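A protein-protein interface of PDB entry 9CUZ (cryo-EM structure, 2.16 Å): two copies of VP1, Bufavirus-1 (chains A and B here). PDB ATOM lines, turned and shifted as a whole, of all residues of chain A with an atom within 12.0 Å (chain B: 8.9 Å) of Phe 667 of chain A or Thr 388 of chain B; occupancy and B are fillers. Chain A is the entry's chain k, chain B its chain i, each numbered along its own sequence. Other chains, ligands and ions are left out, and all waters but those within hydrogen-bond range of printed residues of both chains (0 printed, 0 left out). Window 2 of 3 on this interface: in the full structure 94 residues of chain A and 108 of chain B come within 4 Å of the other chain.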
ATOM      1  N   TRP A 419      40.395  10.078  -2.955  1.00  0.00           N
ATOM      2  CA  TRP A 419      40.862  10.973  -1.913  1.00  0.00           C
ATOM      3  C   TRP A 419      40.578  10.482  -0.500  1.00  0.00           C
ATOM      4  O   TRP A 419      41.099  11.067   0.449  1.00  0.00           O
ATOM      5  CB  TRP A 419      40.228  12.352  -2.112  1.00  0.00           C
ATOM      6  CG  TRP A 419      38.738  12.304  -2.203  1.00  0.00           C
ATOM      7  CD1 TRP A 419      38.002  12.113  -3.325  1.00  0.00           C
ATOM      8  CD2 TRP A 419      37.803  12.440  -1.131  1.00  0.00           C
ATOM      9  NE1 TRP A 419      36.672  12.126  -3.029  1.00  0.00           N
ATOM     10  CE2 TRP A 419      36.517  12.326  -1.686  1.00  0.00           C
ATOM     11  CE3 TRP A 419      37.926  12.650   0.243  1.00  0.00           C
ATOM     12  CZ2 TRP A 419      35.360  12.421  -0.918  1.00  0.00           C
ATOM     13  CZ3 TRP A 419      36.778  12.747   1.001  1.00  0.00           C
ATOM     14  CH2 TRP A 419      35.513  12.633   0.419  1.00  0.00           C
ATOM     15  N   LEU A 663      29.280   9.864 -15.721  1.00  0.00           N
ATOM     16  CA  LEU A 663      28.211  10.829 -15.531  1.00  0.00           C
ATOM     17  C   LEU A 663      28.410  11.561 -14.212  1.00  0.00           C
ATOM     18  O   LEU A 663      28.994  11.009 -13.273  1.00  0.00           O
ATOM     19  CB  LEU A 663      26.832  10.155 -15.541  1.00  0.00           C
ATOM     20  CG  LEU A 663      26.351   9.494 -16.834  1.00  0.00           C
ATOM     21  CD1 LEU A 663      25.028   8.803 -16.630  1.00  0.00           C
ATOM     22  CD2 LEU A 663      26.282  10.488 -17.959  1.00  0.00           C
ATOM     23  N   PRO A 664      27.938  12.802 -14.099  1.00  0.00           N
ATOM     24  CA  PRO A 664      28.203  13.577 -12.878  1.00  0.00           C
ATOM     25  C   PRO A 664      27.615  12.906 -11.646  1.00  0.00           C
ATOM     26  O   PRO A 664      26.443  12.538 -11.620  1.00  0.00           O
ATOM     27  CB  PRO A 664      27.511  14.915 -13.162  1.00  0.00           C
ATOM     28  CG  PRO A 664      27.480  15.012 -14.622  1.00  0.00           C
ATOM     29  CD  PRO A 664      27.280  13.624 -15.129  1.00  0.00           C
ATOM     30  N   ARG A 665      28.453  12.713 -10.636  1.00  0.00           N
ATOM     31  CA  ARG A 665      28.006  12.222  -9.340  1.00  0.00           C
ATOM     32  C   ARG A 665      27.845  13.323  -8.297  1.00  0.00           C
ATOM     33  O   ARG A 665      27.593  13.025  -7.128  1.00  0.00           O
ATOM     34  CB  ARG A 665      28.922  11.119  -8.826  1.00  0.00           C
ATOM     35  CG  ARG A 665      28.858   9.878  -9.683  1.00  0.00           C
ATOM     36  CD  ARG A 665      29.649   8.770  -9.050  1.00  0.00           C
ATOM     37  NE  ARG A 665      29.048   8.424  -7.765  1.00  0.00           N
ATOM     38  CZ  ARG A 665      29.545   7.537  -6.913  1.00  0.00           C
ATOM     39  NH1 ARG A 665      28.927   7.303  -5.766  1.00  0.00           N
ATOM     40  NH2 ARG A 665      30.644   6.871  -7.215  1.00  0.00           N
ATOM     41  N   GLN A 666      28.042  14.576  -8.676  1.00  0.00           N
ATOM     42  CA  GLN A 666      28.029  15.669  -7.721  1.00  0.00           C
ATOM     43  C   GLN A 666      27.241  16.826  -8.310  1.00  0.00           C
ATOM     44  O   GLN A 666      26.936  16.856  -9.500  1.00  0.00           O
ATOM     45  CB  GLN A 666      29.454  16.092  -7.372  1.00  0.00           C
ATOM     46  CG  GLN A 666      30.198  16.662  -8.555  1.00  0.00           C
ATOM     47  CD  GLN A 666      31.639  16.965  -8.254  1.00  0.00           C
ATOM     48  OE1 GLN A 666      32.222  16.386  -7.359  1.00  0.00           O
ATOM     49  NE2 GLN A 666      32.209  17.907  -8.978  1.00  0.00           N
ATOM     50  N   PHE A 667      26.901  17.778  -7.449  1.00  0.00           N
ATOM     51  CA  PHE A 667      26.227  19.010  -7.829  1.00  0.00           C
ATOM     52  C   PHE A 667      27.200  20.014  -8.444  1.00  0.00           C
ATOM     53  O   PHE A 667      26.897  20.620  -9.473  1.00  0.00           O
ATOM     54  CB  PHE A 667      25.570  19.620  -6.591  1.00  0.00           C
ATOM     55  CG  PHE A 667      24.773  20.866  -6.845  1.00  0.00           C
ATOM     56  CD1 PHE A 667      23.424  20.793  -7.149  1.00  0.00           C
ATOM     57  CD2 PHE A 667      25.374  22.105  -6.801  1.00  0.00           C
ATOM     58  CE1 PHE A 667      22.685  21.939  -7.353  1.00  0.00           C
ATOM     59  CE2 PHE A 667      24.643  23.249  -7.030  1.00  0.00           C
ATOM     60  CZ  PHE A 667      23.297  23.165  -7.306  1.00  0.00           C
ATOM     61  N   ASN A 668      28.359  20.197  -7.819  1.00  0.00           N
ATOM     62  CA  ASN A 668      29.309  21.222  -8.215  1.00  0.00           C
ATOM     63  C   ASN A 668      30.122  20.804  -9.442  1.00  0.00           C
ATOM     64  O   ASN A 668      30.052  19.675  -9.922  1.00  0.00           O
ATOM     65  CB  ASN A 668      30.266  21.546  -7.067  1.00  0.00           C
ATOM     66  CG  ASN A 668      30.919  20.305  -6.476  1.00  0.00           C
ATOM     67  OD1 ASN A 668      30.338  19.229  -6.483  1.00  0.00           O
ATOM     68  ND2 ASN A 668      32.168  20.431  -6.077  1.00  0.00           N
ATOM     69  N   LEU A 669      30.953  21.734  -9.906  1.00  0.00           N
ATOM     70  CA  LEU A 669      31.752  21.526 -11.108  1.00  0.00           C
ATOM     71  C   LEU A 669      32.946  20.622 -10.839  1.00  0.00           C
ATOM     72  O   LEU A 669      33.610  20.731  -9.808  1.00  0.00           O
ATOM     73  CB  LEU A 669      32.252  22.859 -11.653  1.00  0.00           C
ATOM     74  CG  LEU A 669      31.257  23.865 -12.222  1.00  0.00           C
ATOM     75  CD1 LEU A 669      31.971  25.152 -12.529  1.00  0.00           C
ATOM     76  CD2 LEU A 669      30.621  23.300 -13.473  1.00  0.00           C
ATOM     77  N   TYR A 670      33.211  19.720 -11.771  1.00  0.00           N
ATOM     78  CA  TYR A 670      34.451  18.961 -11.795  1.00  0.00           C
ATOM     79  C   TYR A 670      35.610  19.780 -12.352  1.00  0.00           C
ATOM     80  O   TYR A 670      35.426  20.759 -13.074  1.00  0.00           O
ATOM     81  CB  TYR A 670      34.302  17.680 -12.606  1.00  0.00           C
ATOM     82  CG  TYR A 670      33.449  16.625 -11.974  1.00  0.00           C
ATOM     83  CD1 TYR A 670      33.997  15.732 -11.067  1.00  0.00           C
ATOM     84  CD2 TYR A 670      32.115  16.490 -12.303  1.00  0.00           C
ATOM     85  CE1 TYR A 670      33.236  14.757 -10.488  1.00  0.00           C
ATOM     86  CE2 TYR A 670      31.344  15.509 -11.727  1.00  0.00           C
ATOM     87  CZ  TYR A 670      31.912  14.642 -10.823  1.00  0.00           C
ATOM     88  OH  TYR A 670      31.156  13.665 -10.243  1.00  0.00           O
ATOM     89  N   ASN A 671      36.818  19.350 -12.001  1.00  0.00           N
ATOM     90  CA  ASN A 671      38.039  19.764 -12.688  1.00  0.00           C
ATOM     91  C   ASN A 671      38.277  18.738 -13.784  1.00  0.00           C
ATOM     92  O   ASN A 671      38.591  17.579 -13.512  1.00  0.00           O
ATOM     93  CB  ASN A 671      39.219  19.818 -11.730  1.00  0.00           C
ATOM     94  CG  ASN A 671      39.105  20.925 -10.725  1.00  0.00           C
ATOM     95  OD1 ASN A 671      38.484  21.950 -10.974  1.00  0.00           O
ATOM     96  ND2 ASN A 671      39.650  20.692  -9.545  1.00  0.00           N
ATOM     97  N   LEU A 672      38.140  19.163 -15.023  1.00  0.00           N
ATOM     98  CA  LEU A 672      38.189  18.237 -16.133  1.00  0.00           C
ATOM     99  C   LEU A 672      39.625  18.040 -16.613  1.00  0.00           C
ATOM    100  O   LEU A 672      40.465  18.920 -16.442  1.00  0.00           O
ATOM    101  CB  LEU A 672      37.280  18.742 -17.245  1.00  0.00           C
ATOM    102  CG  LEU A 672      35.846  18.213 -17.190  1.00  0.00           C
ATOM    103  CD1 LEU A 672      35.218  18.422 -15.881  1.00  0.00           C
ATOM    104  CD2 LEU A 672      35.028  18.993 -18.160  1.00  0.00           C
ATOM    105  N   PRO A 703      38.068  12.925  -9.072  1.00  0.00           N
ATOM    106  CA  PRO A 703      37.733  12.340  -7.780  1.00  0.00           C
ATOM    107  C   PRO A 703      36.523  11.441  -7.906  1.00  0.00           C
ATOM    108  O   PRO A 703      35.631  11.669  -8.723  1.00  0.00           O
ATOM    109  CB  PRO A 703      37.432  13.560  -6.906  1.00  0.00           C
ATOM    110  CG  PRO A 703      36.935  14.572  -7.870  1.00  0.00           C
ATOM    111  CD  PRO A 703      37.716  14.355  -9.131  1.00  0.00           C
ATOM    112  N   ASN A 704      36.519  10.389  -7.106  1.00  0.00           N
ATOM    113  CA  ASN A 704      35.346   9.553  -6.939  1.00  0.00           C
ATOM    114  C   ASN A 704      35.354   9.059  -5.504  1.00  0.00           C
ATOM    115  O   ASN A 704      36.387   9.071  -4.838  1.00  0.00           O
ATOM    116  CB  ASN A 704      35.333   8.386  -7.934  1.00  0.00           C
ATOM    117  CG  ASN A 704      33.978   7.715  -8.034  1.00  0.00           C
ATOM    118  OD1 ASN A 704      32.944   8.353  -7.874  1.00  0.00           O
ATOM    119  ND2 ASN A 704      33.981   6.427  -8.308  1.00  0.00           N
ATOM    120  N   TYR A 705      34.188   8.655  -5.019  1.00  0.00           N
ATOM    121  CA  TYR A 705      34.093   8.108  -3.676  1.00  0.00           C
ATOM    122  C   TYR A 705      34.642   6.689  -3.652  1.00  0.00           C
ATOM    123  O   TYR A 705      34.448   5.922  -4.595  1.00  0.00           O
ATOM    124  CB  TYR A 705      32.646   8.115  -3.187  1.00  0.00           C
ATOM    125  CG  TYR A 705      32.042   9.488  -3.046  1.00  0.00           C
ATOM    126  CD1 TYR A 705      32.259  10.245  -1.909  1.00  0.00           C
ATOM    127  CD2 TYR A 705      31.225  10.013  -4.035  1.00  0.00           C
ATOM    128  CE1 TYR A 705      31.707  11.492  -1.773  1.00  0.00           C
ATOM    129  CE2 TYR A 705      30.664  11.263  -3.903  1.00  0.00           C
ATOM    130  CZ  TYR A 705      30.907  11.995  -2.770  1.00  0.00           C
ATOM    131  OH  TYR A 705      30.350  13.236  -2.635  1.00  0.00           O
ATOM    132  N   TYR B 213      22.055  22.784   3.106  1.00  0.00           N
ATOM    133  CA  TYR B 213      23.278  21.998   3.165  1.00  0.00           C
ATOM    134  C   TYR B 213      24.430  22.885   3.616  1.00  0.00           C
ATOM    135  O   TYR B 213      24.580  24.006   3.133  1.00  0.00           O
ATOM    136  CB  TYR B 213      23.580  21.394   1.798  1.00  0.00           C
ATOM    137  CG  TYR B 213      22.623  20.331   1.343  1.00  0.00           C
ATOM    138  CD1 TYR B 213      22.892  18.993   1.570  1.00  0.00           C
ATOM    139  CD2 TYR B 213      21.425  20.663   0.721  1.00  0.00           C
ATOM    140  CE1 TYR B 213      22.028  18.022   1.154  1.00  0.00           C
ATOM    141  CE2 TYR B 213      20.551  19.697   0.312  1.00  0.00           C
ATOM    142  CZ  TYR B 213      20.859  18.374   0.536  1.00  0.00           C
ATOM    143  OH  TYR B 213      19.999  17.401   0.131  1.00  0.00           O
ATOM    144  N   TRP B 248      18.669  16.068   5.903  1.00  0.00           N
ATOM    145  CA  TRP B 248      18.040  14.756   5.912  1.00  0.00           C
ATOM    146  C   TRP B 248      18.439  13.925   7.133  1.00  0.00           C
ATOM    147  O   TRP B 248      19.504  14.117   7.714  1.00  0.00           O
ATOM    148  CB  TRP B 248      18.404  14.030   4.623  1.00  0.00           C
ATOM    149  CG  TRP B 248      17.773  14.663   3.429  1.00  0.00           C
ATOM    150  CD1 TRP B 248      18.260  15.704   2.708  1.00  0.00           C
ATOM    151  CD2 TRP B 248      16.569  14.261   2.782  1.00  0.00           C
ATOM    152  NE1 TRP B 248      17.423  15.999   1.674  1.00  0.00           N
ATOM    153  CE2 TRP B 248      16.376  15.122   1.691  1.00  0.00           C
ATOM    154  CE3 TRP B 248      15.626  13.259   3.026  1.00  0.00           C
ATOM    155  CZ2 TRP B 248      15.284  15.016   0.851  1.00  0.00           C
ATOM    156  CZ3 TRP B 248      14.551  13.154   2.191  1.00  0.00           C
ATOM    157  CH2 TRP B 248      14.384  14.029   1.116  1.00  0.00           C
ATOM    158  N   GLN B 322      24.419   5.985  -4.968  1.00  0.00           N
ATOM    159  CA  GLN B 322      25.088   7.172  -5.472  1.00  0.00           C
ATOM    160  C   GLN B 322      25.515   8.129  -4.368  1.00  0.00           C
ATOM    161  O   GLN B 322      26.361   8.988  -4.613  1.00  0.00           O
ATOM    162  CB  GLN B 322      24.184   7.900  -6.468  1.00  0.00           C
ATOM    163  CG  GLN B 322      23.877   7.084  -7.702  1.00  0.00           C
ATOM    164  CD  GLN B 322      25.131   6.670  -8.446  1.00  0.00           C
ATOM    165  OE1 GLN B 322      26.056   7.458  -8.622  1.00  0.00           O
ATOM    166  NE2 GLN B 322      25.182   5.415  -8.853  1.00  0.00           N
ATOM    167  N   LEU B 323      24.982   8.006  -3.206  1.00  0.00           N
ATOM    168  CA  LEU B 323      25.322   8.838  -2.064  1.00  0.00           C
ATOM    169  C   LEU B 323      26.460   8.222  -1.259  1.00  0.00           C
ATOM    170  O   LEU B 323      26.620   7.004  -1.244  1.00  0.00           O
ATOM    171  CB  LEU B 323      24.103   9.016  -1.162  1.00  0.00           C
ATOM    172  CG  LEU B 323      22.923   9.748  -1.791  1.00  0.00           C
ATOM    173  CD1 LEU B 323      21.748   9.716  -0.854  1.00  0.00           C
ATOM    174  CD2 LEU B 323      23.298  11.175  -2.135  1.00  0.00           C
ATOM    175  N   TYR B 350      28.240  13.394   5.709  1.00  0.00           N
ATOM    176  CA  TYR B 350      29.369  12.631   5.209  1.00  0.00           C
ATOM    177  C   TYR B 350      30.586  13.536   5.104  1.00  0.00           C
ATOM    178  O   TYR B 350      30.474  14.759   5.100  1.00  0.00           O
ATOM    179  CB  TYR B 350      29.044  11.958   3.870  1.00  0.00           C
ATOM    180  CG  TYR B 350      28.614  12.895   2.766  1.00  0.00           C
ATOM    181  CD1 TYR B 350      29.547  13.503   1.939  1.00  0.00           C
ATOM    182  CD2 TYR B 350      27.269  13.135   2.530  1.00  0.00           C
ATOM    183  CE1 TYR B 350      29.156  14.329   0.917  1.00  0.00           C
ATOM    184  CE2 TYR B 350      26.864  13.970   1.521  1.00  0.00           C
ATOM    185  CZ  TYR B 350      27.807  14.565   0.717  1.00  0.00           C
ATOM    186  OH  TYR B 350      27.404  15.408  -0.272  1.00  0.00           O
ATOM    187  N   LEU B 381      36.746  19.384  -3.846  1.00  0.00           N
ATOM    188  CA  LEU B 381      35.671  18.874  -3.000  1.00  0.00           C
ATOM    189  C   LEU B 381      34.496  18.338  -3.814  1.00  0.00           C
ATOM    190  O   LEU B 381      34.203  18.816  -4.911  1.00  0.00           O
ATOM    191  CB  LEU B 381      35.206  19.975  -2.050  1.00  0.00           C
ATOM    192  CG  LEU B 381      34.203  19.670  -0.940  1.00  0.00           C
ATOM    193  CD1 LEU B 381      34.480  20.542   0.253  1.00  0.00           C
ATOM    194  CD2 LEU B 381      32.792  19.895  -1.437  1.00  0.00           C
ATOM    195  N   GLN B 382      33.816  17.337  -3.265  1.00  0.00           N
ATOM    196  CA  GLN B 382      32.628  16.740  -3.867  1.00  0.00           C
ATOM    197  C   GLN B 382      31.403  17.022  -3.005  1.00  0.00           C
ATOM    198  O   GLN B 382      31.352  16.622  -1.840  1.00  0.00           O
ATOM    199  CB  GLN B 382      32.813  15.243  -4.071  1.00  0.00           C
ATOM    200  CG  GLN B 382      33.783  14.915  -5.171  1.00  0.00           C
ATOM    201  CD  GLN B 382      33.963  13.443  -5.374  1.00  0.00           C
ATOM    202  OE1 GLN B 382      33.920  12.662  -4.441  1.00  0.00           O
ATOM    203  NE2 GLN B 382      34.050  13.046  -6.618  1.00  0.00           N
ATOM    204  N   PHE B 383      30.419  17.694  -3.585  1.00  0.00           N
ATOM    205  CA  PHE B 383      29.173  18.042  -2.915  1.00  0.00           C
ATOM    206  C   PHE B 383      27.996  17.412  -3.642  1.00  0.00           C
ATOM    207  O   PHE B 383      27.663  17.811  -4.759  1.00  0.00           O
ATOM    208  CB  PHE B 383      29.029  19.562  -2.799  1.00  0.00           C
ATOM    209  CG  PHE B 383      27.651  20.024  -2.406  1.00  0.00           C
ATOM    210  CD1 PHE B 383      27.139  19.761  -1.149  1.00  0.00           C
ATOM    211  CD2 PHE B 383      26.917  20.826  -3.260  1.00  0.00           C
ATOM    212  CE1 PHE B 383      25.874  20.204  -0.800  1.00  0.00           C
ATOM    213  CE2 PHE B 383      25.669  21.282  -2.910  1.00  0.00           C
ATOM    214  CZ  PHE B 383      25.146  20.973  -1.679  1.00  0.00           C
ATOM    215  N   THR B 384      27.351  16.446  -2.991  1.00  0.00           N
ATOM    216  CA  THR B 384      26.243  15.697  -3.578  1.00  0.00           C
ATOM    217  C   THR B 384      24.999  15.793  -2.701  1.00  0.00           C
ATOM    218  O   THR B 384      24.825  15.005  -1.757  1.00  0.00           O
ATOM    219  CB  THR B 384      26.640  14.244  -3.869  1.00  0.00           C
ATOM    220  OG1 THR B 384      25.536  13.536  -4.447  1.00  0.00           O
ATOM    221  CG2 THR B 384      27.160  13.505  -2.664  1.00  0.00           C
ATOM    222  N   PRO B 385      24.129  16.761  -2.958  1.00  0.00           N
ATOM    223  CA  PRO B 385      22.878  16.861  -2.204  1.00  0.00           C
ATOM    224  C   PRO B 385      21.904  15.764  -2.602  1.00  0.00           C
ATOM    225  O   PRO B 385      21.991  15.178  -3.678  1.00  0.00           O
ATOM    226  CB  PRO B 385      22.343  18.241  -2.596  1.00  0.00           C
ATOM    227  CG  PRO B 385      22.890  18.461  -3.955  1.00  0.00           C
ATOM    228  CD  PRO B 385      24.240  17.810  -3.982  1.00  0.00           C
ATOM    229  N   ILE B 386      20.965  15.495  -1.698  1.00  0.00           N
ATOM    230  CA  ILE B 386      19.992  14.433  -1.932  1.00  0.00           C
ATOM    231  C   ILE B 386      19.122  14.752  -3.140  1.00  0.00           C
ATOM    232  O   ILE B 386      18.872  13.881  -3.979  1.00  0.00           O
ATOM    233  CB  ILE B 386      19.130  14.213  -0.676  1.00  0.00           C
ATOM    234  CG1 ILE B 386      20.015  13.985   0.552  1.00  0.00           C
ATOM    235  CG2 ILE B 386      18.149  13.077  -0.886  1.00  0.00           C
ATOM    236  CD1 ILE B 386      20.978  12.891   0.411  1.00  0.00           C
ATOM    237  N   GLU B 387      18.676  16.004  -3.264  1.00  0.00           N
ATOM    238  CA  GLU B 387      17.641  16.378  -4.223  1.00  0.00           C
ATOM    239  C   GLU B 387      18.052  16.184  -5.671  1.00  0.00           C
ATOM    240  O   GLU B 387      17.209  15.812  -6.485  1.00  0.00           O
ATOM    241  CB  GLU B 387      17.209  17.823  -3.989  1.00  0.00           C
ATOM    242  CG  GLU B 387      16.417  18.029  -2.713  1.00  0.00           C
ATOM    243  CD  GLU B 387      17.281  18.110  -1.473  1.00  0.00           C
ATOM    244  OE1 GLU B 387      18.506  17.949  -1.588  1.00  0.00           O
ATOM    245  OE2 GLU B 387      16.732  18.334  -0.386  1.00  0.00           O
ATOM    246  N   THR B 388      19.340  16.358  -5.979  1.00  0.00           N
ATOM    247  CA  THR B 388      19.810  16.245  -7.386  1.00  0.00           C
ATOM    248  C   THR B 388      20.351  14.838  -7.648  1.00  0.00           C
ATOM    249  O   THR B 388      20.632  14.529  -8.818  1.00  0.00           O
ATOM    250  CB  THR B 388      20.867  17.308  -7.711  1.00  0.00           C
ATOM    251  OG1 THR B 388      21.971  17.123  -6.825  1.00  0.00           O
ATOM    252  CG2 THR B 388      20.338  18.721  -7.589  1.00  0.00           C
ATOM    253  N   THR B 389      20.482  14.018  -6.604  1.00  0.00           N
ATOM    254  CA  THR B 389      21.097  12.672  -6.771  1.00  0.00           C
ATOM    255  C   THR B 389      20.021  11.584  -6.880  1.00  0.00           C
ATOM    256  O   THR B 389      20.199  10.680  -7.713  1.00  0.00           O
ATOM    257  CB  THR B 389      22.071  12.379  -5.625  1.00  0.00           C
ATOM    258  OG1 THR B 389      23.007  13.453  -5.550  1.00  0.00           O
ATOM    259  CG2 THR B 389      22.806  11.067  -5.794  1.00  0.00           C
ATOM    260  N   THR B 390      18.957  11.658  -6.075  1.00  0.00           N
ATOM    261  CA  THR B 390      17.936  10.575  -6.063  1.00  0.00           C
ATOM    262  C   THR B 390      16.531  11.159  -6.219  1.00  0.00           C
ATOM    263  O   THR B 390      16.356  12.352  -5.920  1.00  0.00           O
ATOM    264  CB  THR B 390      18.011   9.757  -4.766  1.00  0.00           C
ATOM    265  OG1 THR B 390      17.599  10.588  -3.681  1.00  0.00           O
ATOM    266  CG2 THR B 390      19.395   9.211  -4.492  1.00  0.00           C
ATOM    267  N   GLU B 391      15.570  10.343  -6.659  1.00  0.00           N
ATOM    268  CA  GLU B 391      14.158  10.808  -6.739  1.00  0.00           C
ATOM    269  C   GLU B 391      13.585  10.801  -5.321  1.00  0.00           C
ATOM    270  O   GLU B 391      14.034   9.966  -4.515  1.00  0.00           O
ATOM    271  CB  GLU B 391      13.353   9.927  -7.697  1.00  0.00           C
ATOM    272  CG  GLU B 391      13.875   9.977  -9.121  1.00  0.00           C
ATOM    273  CD  GLU B 391      13.067   9.183 -10.131  1.00  0.00           C
ATOM    274  OE1 GLU B 391      12.022   8.626  -9.745  1.00  0.00           O
ATOM    275  OE2 GLU B 391      13.487   9.125 -11.304  1.00  0.00           O
ATOM    276  N   ILE B 392      12.645  11.698  -5.022  1.00  0.00           N
ATOM    277  CA  ILE B 392      12.142  11.815  -3.621  1.00  0.00           C
ATOM    278  C   ILE B 392      10.632  11.579  -3.570  1.00  0.00           C
ATOM    279  O   ILE B 392       9.908  12.224  -4.353  1.00  0.00           O
ATOM    280  CB  ILE B 392      12.512  13.190  -3.028  1.00  0.00           C
ATOM    281  CG1 ILE B 392      14.030  13.394  -2.987  1.00  0.00           C
ATOM    282  CG2 ILE B 392      11.879  13.378  -1.659  1.00  0.00           C
ATOM    283  CD1 ILE B 392      14.451  14.771  -2.532  1.00  0.00           C
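The side-chain hydroxyl (OG1) of Thr 384 of chain B sits at hydrogen-bond distance from the side-chain hydroxyl (OG1) of Thr 389 of chain B (2.8 Å).
The side-chain hydroxyl of Thr 389 of chain B sits at hydrogen-bond distance from the backbone carbonyl oxygen of Pro 385 of chain B (2.7 Å).
N of Arg 665 of chain A lies within hydrogen-bond range of OH of Tyr 670 of chain A, at 2.9 Å.
The guanidinium group of Arg 665 of chain A sits at hydrogen-bond distance from the side-chain amide oxygen of Asn 704 of chain A (2.8 Å).
NE2 of Gln 666 of chain A lies within hydrogen-bond range of O of Asn 668 of chain A (2.9 Å).
The backbone NH of Tyr 670 of chain A sits close to the side-chain amide nitrogen of Gln 666 of chain A.
Leu 663 of chain A touches none of the printed residues of chain B.
Printed residues of chain B within 4 Å of Arg 665 of chain A: Gln 322 (3.3 Å) and Thr 384 (3.4 Å).
Tyr 670 of chain A touches none of the printed residues of chain B.
Of the printed residues of chain A, Tyr 350 of chain B touches Tyr 705 (3.9 Å).
Of the printed residues of chain A, Thr 384 of chain B touches Arg 665 (3.4 Å) and Tyr 705 (3.2 Å).
Pro 385 of chain B touches just one residue of chain A: Phe 667.
No residue of chain A comes within 4 Å of Ile 386 of chain B.
Of chain A, only Phe 667 comes within 4 Å of Thr 388 of chain B.
No residue of chain A comes within 4 Å of Thr 389 of chain B.
No residue of chain A comes within 4 Å of Thr 390 of chain B.
The nearest residue of chain B that does not touch Phe 667 of chain A is Thr 384 of chain B (4.4 Å).
OE1 of Gln 322 of chain B lies within hydrogen-bond range of NE of Arg 665 of chain A, 3.3 Å away.
ND2 of Asn 668 of chain A sits at hydrogen-bond distance from O of Leu 381 of chain B (2.8 Å).
The indole nitrogen of Trp 419 of chain A sits at hydrogen-bond distance from the side-chain amide oxygen of Gln 382 of chain B (3.1 Å).
NE2 of Gln 382 of chain B sits at hydrogen-bond distance from O of Pro 703 of chain A, at 3.0 Å.
The backbone carbonyl oxygen of Phe 383 of chain B sits at hydrogen-bond distance from the backbone NH of Phe 667 of chain A.
The side-chain amide oxygen (OD1) of Asn 668 of chain A lies within hydrogen-bond range of the backbone NH (N) of Phe 383 of chain B.
The side-chain hydroxyl (OG1) of Thr 384 of chain B sits at hydrogen-bond distance from the backbone carbonyl oxygen (O) of Arg 665 of chain A, at 3.4 Å.
Of the 17 printed residues of chain B, 8 touch a printed residue of chain A.
Along chain B the printed residues that touch a printed residue of chain A span positions 322 to 388.
Among the printed residues, no Asp or Glu carboxylate lies within 4 Å of a Lys or Arg side-chain nitrogen of the other chain.
No position is printed for both chains.
Among the printed residues, pairs that only touch across the chains: Gln 666 of chain A with Gln 382 of chain B, Tyr 705 of chain A with Thr 384 of chain B, Phe 667 of chain A with Pro 385 of chain B, Tyr 705 of chain A with Gln 382 of chain B, Gln 666 of chain A with Phe 383 of chain B, Asn 704 of chain A with Gln 382 of chain B, Phe 667 of chain A with Thr 388 of chain B, Tyr 705 of chain A with Tyr 350 of chain B and Gln 666 of chain A with Leu 381 of chain B.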
